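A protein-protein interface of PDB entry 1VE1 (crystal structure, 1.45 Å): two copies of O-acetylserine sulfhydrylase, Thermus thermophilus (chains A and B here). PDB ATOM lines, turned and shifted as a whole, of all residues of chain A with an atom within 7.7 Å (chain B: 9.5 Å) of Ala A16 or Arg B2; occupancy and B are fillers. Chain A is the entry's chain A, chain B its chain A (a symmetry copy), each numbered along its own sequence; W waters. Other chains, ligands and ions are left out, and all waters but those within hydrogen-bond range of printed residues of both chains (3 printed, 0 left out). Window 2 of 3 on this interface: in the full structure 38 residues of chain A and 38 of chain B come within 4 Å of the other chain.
Hydrophobic or aromatic side chains of chain B within 4 Å of the printed part of chain A: Met B1, Val B3, Ala B6, Met B79 and Ala B82. Hydrophobic or aromatic side chains of chain A that line the printed part of chain B: Pro A11, Val A13, Ala A16, Trp A27 and Leu A258. Among the printed residues, 19 pairs touch across the chains. Among the printed residues, no Asp or Glu carboxylate lies within 4 Å of a Lys or Arg side-chain nitrogen of the other chain.
No position is printed for both chains. Of the 19 pairs that touch across the chains among the printed residues, none has its exchanged pair printed and touching as well.
Of chain B, only Arg B2 comes within 4 Å of Ala A16. Lys A17 touches just these residues of chain B: Arg B2 (3.6 Å), Ala B82 (3.4 Å) and Ser B83 (2.6 Å). Of the printed residues of chain B, Trp A27 touches Met B1. Leu A30 touches none of the printed residues of chain B. Leu A252 touches none of the printed residues of chain B. Arg B2 touches just these residues of chain A: Val A13, Ala A16 and Lys A17. Of the printed residues of chain A, Ser B83 touches Lys A17 (2.6 Å) and Glu A256 (3.6 Å). The nearest printed residue of chain A that does not touch Ala B6 is Val A13 (4.7 Å).
The backbone carbonyl oxygen (O) of Pro A11 lies within hydrogen-bond range of the backbone NH (N) of Leu A30 (2.9 Å). N of Ala A16 lies within hydrogen-bond range of OE2 of Glu A256 (3.0 Å). O of Glu A255 lies within hydrogen-bond range of NZ of Lys A17, at 2.7 Å. N of Lys A17 sits at hydrogen-bond distance from OE1 of Glu A256. The backbone NH (N) of Gly A257 is in hydrogen-bond range of the backbone carbonyl oxygen (O) of Leu A252. The side-chain carboxylate (OE1) of Glu B4 lies within hydrogen-bond range of the side-chain hydroxyl (OG) of Ser B83 (2.6 Å).
The backbone carbonyl oxygen (O) of Met B1 lies within hydrogen-bond range of the backbone NH (N) of Arg A14, 2.8 Å away. NZ of Lys A17 sits at hydrogen-bond distance from O of Ala B82 (3.4 Å). The side-chain amino group of Lys A17 sits at hydrogen-bond distance from the backbone carbonyl oxygen of Ser B83, 2.6 Å away. The backbone carbonyl oxygen (O) of Ala B82 lies close to the backbone carbonyl oxygen (O) of Glu A255 (3.2 Å).
Water W3 lies within hydrogen-bond range of O of Glu A256 (2.7 Å) and N of Val B3 (2.8 Å). Water W1 bridges O of Gly A257 (2.8 Å) and O of Pro B35 (3.3 Å). Water W2 lies within hydrogen-bond range of the side-chain hydroxyl (OG) of Ser B83 (3.0 Å) and the side-chain amino group (NZ) of Lys A17 (3.4 Å).
Among the printed residues, merely in contact across the chains: Ala A16 with Arg B2 (3.3 Å), Val A13 with Met B1 (3.3 Å), Gly A257 with Met B79 (3.4 Å), Trp A27 with Met B1 (3.5 Å), Val A12 with Met B1 (3.6 Å), Lys A17 with Arg B2 (3.6 Å), Glu A256 with Ser B83 (3.6 Å), Gly A257 with Val B3 (3.7 Å), Glu A256 with Val B3 (3.7 Å), Pro A11 with Ala B6 (3.8 Å), Gly A257 with Ala B82 (3.8 Å), Val A13 with Arg B2 (3.9 Å), Leu A258 with Val B3 (3.9 Å), Val A13 with Val B3 (3.96 Å) and Pro A11 with Met B1 (3.997 Å).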
ATOM      1  N   PRO A  11       1.990  24.804  -1.752  1.00  0.00           N
ATOM      2  CA  PRO A  11       2.030  24.141  -3.059  1.00  0.00           C
ATOM      3  C   PRO A  11       1.919  22.623  -3.008  1.00  0.00           C
ATOM      4  O   PRO A  11       2.122  21.999  -1.964  1.00  0.00           O
ATOM      5  CB  PRO A  11       3.369  24.596  -3.620  1.00  0.00           C
ATOM      6  CG  PRO A  11       4.231  24.583  -2.397  1.00  0.00           C
ATOM      7  CD  PRO A  11       3.342  25.224  -1.336  1.00  0.00           C
ATOM      8  N   VAL A  12       1.586  22.034  -4.152  1.00  0.00           N
ATOM      9  CA  VAL A  12       1.480  20.590  -4.275  1.00  0.00           C
ATOM     10  C   VAL A  12       2.371  20.182  -5.445  1.00  0.00           C
ATOM     11  O   VAL A  12       2.292  20.767  -6.528  1.00  0.00           O
ATOM     12  CB  VAL A  12       0.015  20.139  -4.531  1.00  0.00           C
ATOM     13  CG1 VAL A  12      -0.485  20.672  -5.863  1.00  0.00           C
ATOM     14  CG2 VAL A  12      -0.077  18.625  -4.477  1.00  0.00           C
ATOM     15  N   VAL A  13       3.238  19.203  -5.215  1.00  0.00           N
ATOM     16  CA  VAL A  13       4.144  18.736  -6.255  1.00  0.00           C
ATOM     17  C   VAL A  13       3.850  17.296  -6.641  1.00  0.00           C
ATOM     18  O   VAL A  13       3.361  16.507  -5.830  1.00  0.00           O
ATOM     19  CB  VAL A  13       5.615  18.829  -5.798  1.00  0.00           C
ATOM     20  CG1 VAL A  13       5.993  20.282  -5.553  1.00  0.00           C
ATOM     21  CG2 VAL A  13       5.821  18.006  -4.544  1.00  0.00           C
ATOM     22  N   ARG A  14       4.149  16.954  -7.889  1.00  0.00           N
ATOM     23  CA  ARG A  14       3.926  15.602  -8.374  1.00  0.00           C
ATOM     24  C   ARG A  14       5.247  14.845  -8.426  1.00  0.00           C
ATOM     25  O   ARG A  14       6.199  15.287  -9.071  1.00  0.00           O
ATOM     26  CB  ARG A  14       3.304  15.623  -9.771  1.00  0.00           C
ATOM     27  CG  ARG A  14       3.088  14.231 -10.327  1.00  0.00           C
ATOM     28  CD  ARG A  14       2.523  14.239 -11.733  1.00  0.00           C
ATOM     29  NE  ARG A  14       2.535  12.889 -12.287  1.00  0.00           N
ATOM     30  CZ  ARG A  14       2.153  12.583 -13.522  1.00  0.00           C
ATOM     31  NH1 ARG A  14       1.722  13.534 -14.339  1.00  0.00           N
ATOM     32  NH2 ARG A  14       2.220  11.327 -13.943  1.00  0.00           N
ATOM     33  N   LEU A  15       5.302  13.707  -7.744  1.00  0.00           N
ATOM     34  CA  LEU A  15       6.512  12.894  -7.725  1.00  0.00           C
ATOM     35  C   LEU A  15       6.803  12.375  -9.131  1.00  0.00           C
ATOM     36  O   LEU A  15       5.882  12.034  -9.876  1.00  0.00           O
ATOM     37  CB  LEU A  15       6.351  11.726  -6.751  1.00  0.00           C
ATOM     38  CG  LEU A  15       6.013  12.138  -5.312  1.00  0.00           C
ATOM     39  CD1 LEU A  15       6.013  10.907  -4.423  1.00  0.00           C
ATOM     40  CD2 LEU A  15       7.028  13.156  -4.809  1.00  0.00           C
ATOM     41  N   ALA A  16       8.084  12.306  -9.482  1.00  0.00           N
ATOM     42  CA  ALA A  16       8.474  11.856 -10.816  1.00  0.00           C
ATOM     43  C   ALA A  16       9.583  10.809 -10.860  1.00  0.00           C
ATOM     44  O   ALA A  16       9.799  10.186 -11.901  1.00  0.00           O
ATOM     45  CB  ALA A  16       8.881  13.062 -11.656  1.00  0.00           C
ATOM     46  N   LYS A  17      10.281  10.600  -9.749  1.00  0.00           N
ATOM     47  CA  LYS A  17      11.377   9.634  -9.739  1.00  0.00           C
ATOM     48  C   LYS A  17      11.188   8.411  -8.852  1.00  0.00           C
ATOM     49  O   LYS A  17      11.597   7.312  -9.222  1.00  0.00           O
ATOM     50  CB  LYS A  17      12.692  10.325  -9.360  1.00  0.00           C
ATOM     51  CG  LYS A  17      13.209  11.324 -10.389  1.00  0.00           C
ATOM     52  CD  LYS A  17      12.349  12.582 -10.425  1.00  0.00           C
ATOM     53  CE  LYS A  17      13.016  13.678 -11.229  1.00  0.00           C
ATOM     54  NZ  LYS A  17      14.356  14.004 -10.674  1.00  0.00           N
ATOM     55  N   VAL A  18      10.588   8.590  -7.679  1.00  0.00           N
ATOM     56  CA  VAL A  18      10.379   7.460  -6.778  1.00  0.00           C
ATOM     57  C   VAL A  18       9.152   6.645  -7.175  1.00  0.00           C
ATOM     58  O   VAL A  18       8.903   5.568  -6.627  1.00  0.00           O
ATOM     59  CB  VAL A  18      10.234   7.921  -5.303  1.00  0.00           C
ATOM     60  CG1 VAL A  18      11.504   8.639  -4.861  1.00  0.00           C
ATOM     61  CG2 VAL A  18       9.026   8.825  -5.147  1.00  0.00           C
ATOM     62  N   VAL A  19       8.387   7.162  -8.132  1.00  0.00           N
ATOM     63  CA  VAL A  19       7.205   6.463  -8.616  1.00  0.00           C
ATOM     64  C   VAL A  19       7.595   5.584  -9.796  1.00  0.00           C
ATOM     65  O   VAL A  19       8.680   5.732 -10.361  1.00  0.00           O
ATOM     66  CB  VAL A  19       6.102   7.445  -9.070  1.00  0.00           C
ATOM     67  CG1 VAL A  19       5.518   8.159  -7.865  1.00  0.00           C
ATOM     68  CG2 VAL A  19       6.671   8.456 -10.052  1.00  0.00           C
ATOM     69  N   GLU A  20       6.707   4.661 -10.148  1.00  0.00           N
ATOM     70  CA  GLU A  20       6.928   3.744 -11.259  1.00  0.00           C
ATOM     71  C   GLU A  20       5.767   3.907 -12.237  1.00  0.00           C
ATOM     72  O   GLU A  20       4.683   4.342 -11.854  1.00  0.00           O
ATOM     73  CB  GLU A  20       7.002   2.309 -10.738  1.00  0.00           C
ATOM     74  CG  GLU A  20       8.161   2.076  -9.775  1.00  0.00           C
ATOM     75  CD  GLU A  20       8.074   0.743  -9.064  1.00  0.00           C
ATOM     76  OE1 GLU A  20       8.091  -0.301  -9.747  1.00  0.00           O
ATOM     77  OE2 GLU A  20       7.990   0.740  -7.817  1.00  0.00           O
ATOM     78  N   VAL A  26       1.150  10.576  -8.032  1.00  0.00           N
ATOM     79  CA  VAL A  26       1.262  10.830  -6.603  1.00  0.00           C
ATOM     80  C   VAL A  26       1.620  12.294  -6.393  1.00  0.00           C
ATOM     81  O   VAL A  26       2.675  12.764  -6.835  1.00  0.00           O
ATOM     82  CB  VAL A  26       2.329   9.945  -5.928  1.00  0.00           C
ATOM     83  CG1 VAL A  26       2.429  10.302  -4.445  1.00  0.00           C
ATOM     84  CG2 VAL A  26       1.963   8.474  -6.079  1.00  0.00           C
ATOM     85  N   TRP A  27       0.716  13.014  -5.736  1.00  0.00           N
ATOM     86  CA  TRP A  27       0.903  14.430  -5.453  1.00  0.00           C
ATOM     87  C   TRP A  27       1.103  14.646  -3.956  1.00  0.00           C
ATOM     88  O   TRP A  27       0.419  14.036  -3.131  1.00  0.00           O
ATOM     89  CB  TRP A  27      -0.303  15.230  -5.946  1.00  0.00           C
ATOM     90  CG  TRP A  27      -0.446  15.228  -7.437  1.00  0.00           C
ATOM     91  CD1 TRP A  27      -0.899  14.205  -8.221  1.00  0.00           C
ATOM     92  CD2 TRP A  27      -0.116  16.300  -8.325  1.00  0.00           C
ATOM     93  NE1 TRP A  27      -0.872  14.575  -9.546  1.00  0.00           N
ATOM     94  CE2 TRP A  27      -0.395  15.856  -9.638  1.00  0.00           C
ATOM     95  CE3 TRP A  27       0.390  17.594  -8.140  1.00  0.00           C
ATOM     96  CZ2 TRP A  27      -0.186  16.666 -10.762  1.00  0.00           C
ATOM     97  CZ3 TRP A  27       0.598  18.398  -9.257  1.00  0.00           C
ATOM     98  CH2 TRP A  27       0.309  17.927 -10.552  1.00  0.00           C
ATOM     99  N   LEU A  30       3.025  20.369   0.315  1.00  0.00           N
ATOM    100  CA  LEU A  30       4.135  20.722   1.200  1.00  0.00           C
ATOM    101  C   LEU A  30       3.797  21.686   2.329  1.00  0.00           C
ATOM    102  O   LEU A  30       3.955  22.900   2.198  1.00  0.00           O
ATOM    103  CB  LEU A  30       5.278  21.294   0.355  1.00  0.00           C
ATOM    104  CG  LEU A  30       5.665  20.446  -0.866  1.00  0.00           C
ATOM    105  CD1 LEU A  30       6.767  21.140  -1.651  1.00  0.00           C
ATOM    106  CD2 LEU A  30       6.114  19.067  -0.409  1.00  0.00           C
ATOM    107  N   LEU A 252      13.531  10.774  -1.660  1.00  0.00           N
ATOM    108  CA  LEU A 252      12.737  11.942  -2.020  1.00  0.00           C
ATOM    109  C   LEU A 252      13.617  13.184  -2.071  1.00  0.00           C
ATOM    110  O   LEU A 252      13.486  14.019  -2.967  1.00  0.00           O
ATOM    111  CB  LEU A 252      11.608  12.155  -1.008  1.00  0.00           C
ATOM    112  CG  LEU A 252      10.454  11.149  -1.041  1.00  0.00           C
ATOM    113  CD1 LEU A 252       9.542  11.373   0.154  1.00  0.00           C
ATOM    114  CD2 LEU A 252       9.672  11.318  -2.334  1.00  0.00           C
ATOM    115  N   GLU A 255      16.331  12.536  -5.078  1.00  0.00           N
ATOM    116  CA  GLU A 255      15.781  12.320  -6.411  1.00  0.00           C
ATOM    117  C   GLU A 255      14.654  13.269  -6.814  1.00  0.00           C
ATOM    118  O   GLU A 255      14.395  13.455  -8.001  1.00  0.00           O
ATOM    119  CB  GLU A 255      15.301  10.870  -6.540  1.00  0.00           C
ATOM    120  CG  GLU A 255      16.416   9.841  -6.404  1.00  0.00           C
ATOM    121  CD  GLU A 255      15.903   8.418  -6.446  1.00  0.00           C
ATOM    122  OE1 GLU A 255      15.049   8.120  -7.307  1.00  0.00           O
ATOM    123  OE2 GLU A 255      16.360   7.598  -5.623  1.00  0.00           O
ATOM    124  N   GLU A 256      13.984  13.867  -5.836  1.00  0.00           N
ATOM    125  CA  GLU A 256      12.890  14.790  -6.137  1.00  0.00           C
ATOM    126  C   GLU A 256      13.195  16.204  -5.649  1.00  0.00           C
ATOM    127  O   GLU A 256      12.488  17.144  -5.999  1.00  0.00           O
ATOM    128  CB  GLU A 256      11.585  14.332  -5.472  1.00  0.00           C
ATOM    129  CG  GLU A 256      11.228  12.864  -5.655  1.00  0.00           C
ATOM    130  CD  GLU A 256      10.458  12.564  -6.929  1.00  0.00           C
ATOM    131  OE1 GLU A 256      10.113  11.381  -7.119  1.00  0.00           O
ATOM    132  OE2 GLU A 256      10.190  13.487  -7.728  1.00  0.00           O
ATOM    133  N   GLY A 257      14.245  16.350  -4.846  1.00  0.00           N
ATOM    134  CA  GLY A 257      14.580  17.655  -4.304  1.00  0.00           C
ATOM    135  C   GLY A 257      13.602  18.020  -3.200  1.00  0.00           C
ATOM    136  O   GLY A 257      13.411  19.195  -2.884  1.00  0.00           O
ATOM    137  N   LEU A 258      12.975  17.001  -2.618  1.00  0.00           N
ATOM    138  CA  LEU A 258      12.011  17.201  -1.541  1.00  0.00           C
ATOM    139  C   LEU A 258      12.607  16.712  -0.223  1.00  0.00           C
ATOM    140  O   LEU A 258      12.644  15.515   0.052  1.00  0.00           O
ATOM    141  CB  LEU A 258      10.706  16.457  -1.853  1.00  0.00           C
ATOM    142  CG  LEU A 258       9.977  16.956  -3.111  1.00  0.00           C
ATOM    143  CD1 LEU A 258       8.803  16.039  -3.429  1.00  0.00           C
ATOM    144  CD2 LEU A 258       9.498  18.391  -2.911  1.00  0.00           C
ATOM    145  N   MET B   1       3.360  19.810 -10.906  1.00  0.00           N
ATOM    146  CA  MET B   1       4.652  20.542 -11.016  1.00  0.00           C
ATOM    147  C   MET B   1       5.705  19.950 -10.096  1.00  0.00           C
ATOM    148  O   MET B   1       5.413  19.094  -9.261  1.00  0.00           O
ATOM    149  CB  MET B   1       4.465  22.030 -10.692  1.00  0.00           C
ATOM    150  CG  MET B   1       3.885  22.326  -9.322  1.00  0.00           C
ATOM    151  SD  MET B   1       3.986  24.086  -8.890  1.00  0.00           S
ATOM    152  CE  MET B   1       4.774  23.967  -7.309  1.00  0.00           C
ATOM    153  N   ARG B   2       6.938  20.408 -10.261  1.00  0.00           N
ATOM    154  CA  ARG B   2       8.036  19.921  -9.448  1.00  0.00           C
ATOM    155  C   ARG B   2       8.464  20.976  -8.440  1.00  0.00           C
ATOM    156  O   ARG B   2       7.967  22.101  -8.467  1.00  0.00           O
ATOM    157  CB  ARG B   2       9.184  19.487 -10.356  1.00  0.00           C
ATOM    158  CG  ARG B   2       8.719  18.383 -11.301  1.00  0.00           C
ATOM    159  CD  ARG B   2       9.847  17.718 -12.039  1.00  0.00           C
ATOM    160  NE  ARG B   2       9.352  16.622 -12.868  1.00  0.00           N
ATOM    161  CZ  ARG B   2      10.135  15.806 -13.563  1.00  0.00           C
ATOM    162  NH1 ARG B   2      11.448  15.965 -13.525  1.00  0.00           N
ATOM    163  NH2 ARG B   2       9.606  14.834 -14.297  1.00  0.00           N
ATOM    164  N   VAL B   3       9.389  20.618  -7.556  1.00  0.00           N
ATOM    165  CA  VAL B   3       9.808  21.537  -6.506  1.00  0.00           C
ATOM    166  C   VAL B   3      10.239  22.916  -6.991  1.00  0.00           C
ATOM    167  O   VAL B   3       9.927  23.918  -6.351  1.00  0.00           O
ATOM    168  CB  VAL B   3      10.922  20.914  -5.629  1.00  0.00           C
ATOM    169  CG1 VAL B   3      12.232  20.851  -6.394  1.00  0.00           C
ATOM    170  CG2 VAL B   3      11.067  21.713  -4.336  1.00  0.00           C
ATOM    171  N   GLU B   4      10.945  22.980  -8.117  1.00  0.00           N
ATOM    172  CA  GLU B   4      11.385  24.272  -8.637  1.00  0.00           C
ATOM    173  C   GLU B   4      10.188  25.171  -8.944  1.00  0.00           C
ATOM    174  O   GLU B   4      10.300  26.399  -8.933  1.00  0.00           O
ATOM    175  CB  GLU B   4      12.243  24.094  -9.900  1.00  0.00           C
ATOM    176  CG  GLU B   4      11.595  23.260 -10.998  1.00  0.00           C
ATOM    177  CD  GLU B   4      11.998  21.798 -10.946  1.00  0.00           C
ATOM    178  OE1 GLU B   4      12.295  21.294  -9.842  1.00  0.00           O
ATOM    179  OE2 GLU B   4      12.007  21.144 -12.012  1.00  0.00           O
ATOM    180  N   GLY B   5       9.043  24.553  -9.216  1.00  0.00           N
ATOM    181  CA  GLY B   5       7.846  25.322  -9.505  1.00  0.00           C
ATOM    182  C   GLY B   5       7.243  25.943  -8.258  1.00  0.00           C
ATOM    183  O   GLY B   5       6.405  26.841  -8.350  1.00  0.00           O
ATOM    184  N   ALA B   6       7.673  25.471  -7.089  1.00  0.00           N
ATOM    185  CA  ALA B   6       7.173  25.970  -5.809  1.00  0.00           C
ATOM    186  C   ALA B   6       8.024  27.107  -5.255  1.00  0.00           C
ATOM    187  O   ALA B   6       7.822  27.546  -4.120  1.00  0.00           O
ATOM    188  CB  ALA B   6       7.114  24.834  -4.799  1.00  0.00           C
ATOM    189  N   ILE B   7       8.977  27.574  -6.053  1.00  0.00           N
ATOM    190  CA  ILE B   7       9.858  28.660  -5.640  1.00  0.00           C
ATOM    191  C   ILE B   7       9.190  30.014  -5.847  1.00  0.00           C
ATOM    192  O   ILE B   7       8.553  30.249  -6.869  1.00  0.00           O
ATOM    193  CB  ILE B   7      11.182  28.635  -6.446  1.00  0.00           C
ATOM    194  CG1 ILE B   7      11.995  27.393  -6.074  1.00  0.00           C
ATOM    195  CG2 ILE B   7      11.982  29.909  -6.187  1.00  0.00           C
ATOM    196  CD1 ILE B   7      13.228  27.186  -6.942  1.00  0.00           C
ATOM    197  N   PRO B  35      11.014  26.386  -0.876  1.00  0.00           N
ATOM    198  CA  PRO B  35      11.314  24.968  -0.638  1.00  0.00           C
ATOM    199  C   PRO B  35      12.740  24.629  -0.212  1.00  0.00           C
ATOM    200  O   PRO B  35      12.970  23.622   0.458  1.00  0.00           O
ATOM    201  CB  PRO B  35      10.917  24.304  -1.960  1.00  0.00           C
ATOM    202  CG  PRO B  35      11.135  25.385  -2.965  1.00  0.00           C
ATOM    203  CD  PRO B  35      10.577  26.605  -2.266  1.00  0.00           C
ATOM    204  N   TRP B  45      17.771  28.399  -9.200  1.00  0.00           N
ATOM    205  CA  TRP B  45      16.919  27.948 -10.292  1.00  0.00           C
ATOM    206  C   TRP B  45      17.215  28.748 -11.562  1.00  0.00           C
ATOM    207  O   TRP B  45      17.399  28.172 -12.633  1.00  0.00           O
ATOM    208  CB  TRP B  45      15.442  28.102  -9.900  1.00  0.00           C
ATOM    209  CG  TRP B  45      14.453  27.875 -11.023  1.00  0.00           C
ATOM    210  CD1 TRP B  45      13.348  28.627 -11.293  1.00  0.00           C
ATOM    211  CD2 TRP B  45      14.472  26.825 -12.005  1.00  0.00           C
ATOM    212  NE1 TRP B  45      12.676  28.116 -12.379  1.00  0.00           N
ATOM    213  CE2 TRP B  45      13.343  27.011 -12.835  1.00  0.00           C
ATOM    214  CE3 TRP B  45      15.332  25.750 -12.264  1.00  0.00           C
ATOM    215  CZ2 TRP B  45      13.050  26.159 -13.909  1.00  0.00           C
ATOM    216  CZ3 TRP B  45      15.039  24.902 -13.336  1.00  0.00           C
ATOM    217  CH2 TRP B  45      13.907  25.116 -14.142  1.00  0.00           C
ATOM    218  N   GLU B  52      20.286  25.962 -19.187  1.00  0.00           N
ATOM    219  CA  GLU B  52      19.536  25.034 -20.028  1.00  0.00           C
ATOM    220  C   GLU B  52      19.090  25.782 -21.282  1.00  0.00           C
ATOM    221  O   GLU B  52      19.212  25.276 -22.399  1.00  0.00           O
ATOM    222  CB  GLU B  52      18.315  24.488 -19.271  1.00  0.00           C
ATOM    223  CG  GLU B  52      18.679  23.620 -18.066  1.00  0.00           C
ATOM    224  CD  GLU B  52      17.468  23.116 -17.299  1.00  0.00           C
ATOM    225  OE1 GLU B  52      16.337  23.541 -17.611  1.00  0.00           O
ATOM    226  OE2 GLU B  52      17.654  22.296 -16.373  1.00  0.00           O
ATOM    227  N   PRO B  59      18.271  18.995 -18.836  1.00  0.00           N
ATOM    228  CA  PRO B  59      17.905  18.239 -17.633  1.00  0.00           C
ATOM    229  C   PRO B  59      17.826  16.727 -17.813  1.00  0.00           C
ATOM    230  O   PRO B  59      17.534  16.232 -18.903  1.00  0.00           O
ATOM    231  CB  PRO B  59      16.571  18.867 -17.232  1.00  0.00           C
ATOM    232  CG  PRO B  59      15.970  19.237 -18.547  1.00  0.00           C
ATOM    233  CD  PRO B  59      17.148  19.827 -19.301  1.00  0.00           C
ATOM    234  N   GLY B  60      18.107  16.004 -16.730  1.00  0.00           N
ATOM    235  CA  GLY B  60      18.068  14.551 -16.753  1.00  0.00           C
ATOM    236  C   GLY B  60      19.287  13.940 -17.417  1.00  0.00           C
ATOM    237  O   GLY B  60      19.336  12.734 -17.653  1.00  0.00           O
ATOM    238  N   MET B  79      19.082  21.254  -4.293  1.00  0.00           N
ATOM    239  CA  MET B  79      17.672  20.937  -4.459  1.00  0.00           C
ATOM    240  C   MET B  79      17.327  20.850  -5.942  1.00  0.00           C
ATOM    241  O   MET B  79      16.695  19.888  -6.386  1.00  0.00           O
ATOM    242  CB  MET B  79      16.822  22.010  -3.786  1.00  0.00           C
ATOM    243  CG  MET B  79      15.328  21.824  -3.981  1.00  0.00           C
ATOM    244  SD  MET B  79      14.396  23.133  -3.166  1.00  0.00           S
ATOM    245  CE  MET B  79      14.653  24.484  -4.318  1.00  0.00           C
ATOM    246  N   ILE B  80      17.738  21.854  -6.710  1.00  0.00           N
ATOM    247  CA  ILE B  80      17.451  21.862  -8.141  1.00  0.00           C
ATOM    248  C   ILE B  80      18.175  20.726  -8.866  1.00  0.00           C
ATOM    249  O   ILE B  80      17.592  20.075  -9.730  1.00  0.00           O
ATOM    250  CB  ILE B  80      17.836  23.212  -8.787  1.00  0.00           C
ATOM    251  CG1 ILE B  80      17.050  24.355  -8.135  1.00  0.00           C
ATOM    252  CG2 ILE B  80      17.542  23.176 -10.283  1.00  0.00           C
ATOM    253  CD1 ILE B  80      15.549  24.275  -8.331  1.00  0.00           C
ATOM    254  N   ALA B  81      19.436  20.483  -8.516  1.00  0.00           N
ATOM    255  CA  ALA B  81      20.191  19.409  -9.158  1.00  0.00           C
ATOM    256  C   ALA B  81      19.515  18.065  -8.887  1.00  0.00           C
ATOM    257  O   ALA B  81      19.472  17.195  -9.754  1.00  0.00           O
ATOM    258  CB  ALA B  81      21.630  19.390  -8.640  1.00  0.00           C
ATOM    259  N   ALA B  82      18.986  17.891  -7.680  1.00  0.00           N
ATOM    260  CA  ALA B  82      18.305  16.648  -7.336  1.00  0.00           C
ATOM    261  C   ALA B  82      17.044  16.488  -8.178  1.00  0.00           C
ATOM    262  O   ALA B  82      16.797  15.430  -8.755  1.00  0.00           O
ATOM    263  CB  ALA B  82      17.945  16.641  -5.847  1.00  0.00           C
ATOM    264  N   SER B  83      16.252  17.548  -8.257  1.00  0.00           N
ATOM    265  CA  SER B  83      15.010  17.506  -9.017  1.00  0.00           C
ATOM    266  C   SER B  83      15.198  17.343 -10.523  1.00  0.00           C
ATOM    267  O   SER B  83      14.458  16.597 -11.166  1.00  0.00           O
ATOM    268  CB  SER B  83      14.195  18.773  -8.756  1.00  0.00           C
ATOM    269  OG  SER B  83      12.985  18.759  -9.500  1.00  0.00           O
ATOM    270  N   ARG B  84      16.190  18.027 -11.083  1.00  0.00           N
ATOM    271  CA  ARG B  84      16.403  17.969 -12.522  1.00  0.00           C
ATOM    272  C   ARG B  84      17.459  17.004 -13.043  1.00  0.00           C
ATOM    273  O   ARG B  84      17.779  17.011 -14.233  1.00  0.00           O
ATOM    274  CB  ARG B  84      16.644  19.378 -13.044  1.00  0.00           C
ATOM    275  CG  ARG B  84      15.475  20.295 -12.714  1.00  0.00           C
ATOM    276  CD  ARG B  84      15.668  21.678 -13.270  1.00  0.00           C
ATOM    277  NE  ARG B  84      15.440  21.750 -14.711  1.00  0.00           N
ATOM    278  CZ  ARG B  84      14.243  21.688 -15.286  1.00  0.00           C
ATOM    279  NH1 ARG B  84      13.150  21.539 -14.547  1.00  0.00           N
ATOM    280  NH2 ARG B  84      14.135  21.819 -16.602  1.00  0.00           N
ATOM    281  N   GLY B  85      18.001  16.178 -12.159  1.00  0.00           N
ATOM    282  CA  GLY B  85      18.960  15.171 -12.579  1.00  0.00           C
ATOM    283  C   GLY B  85      20.376  15.566 -12.941  1.00  0.00           C
ATOM    284  O   GLY B  85      20.936  15.039 -13.905  1.00  0.00           O
HETATM  285  O   HOH W   1      12.807  20.504  -0.497  1.00  0.00           O
HETATM  286  O   HOH W   2      11.810  16.021  -9.561  1.00  0.00           O
HETATM  287  O   HOH W   3      10.248  17.929  -7.268  1.00  0.00           O
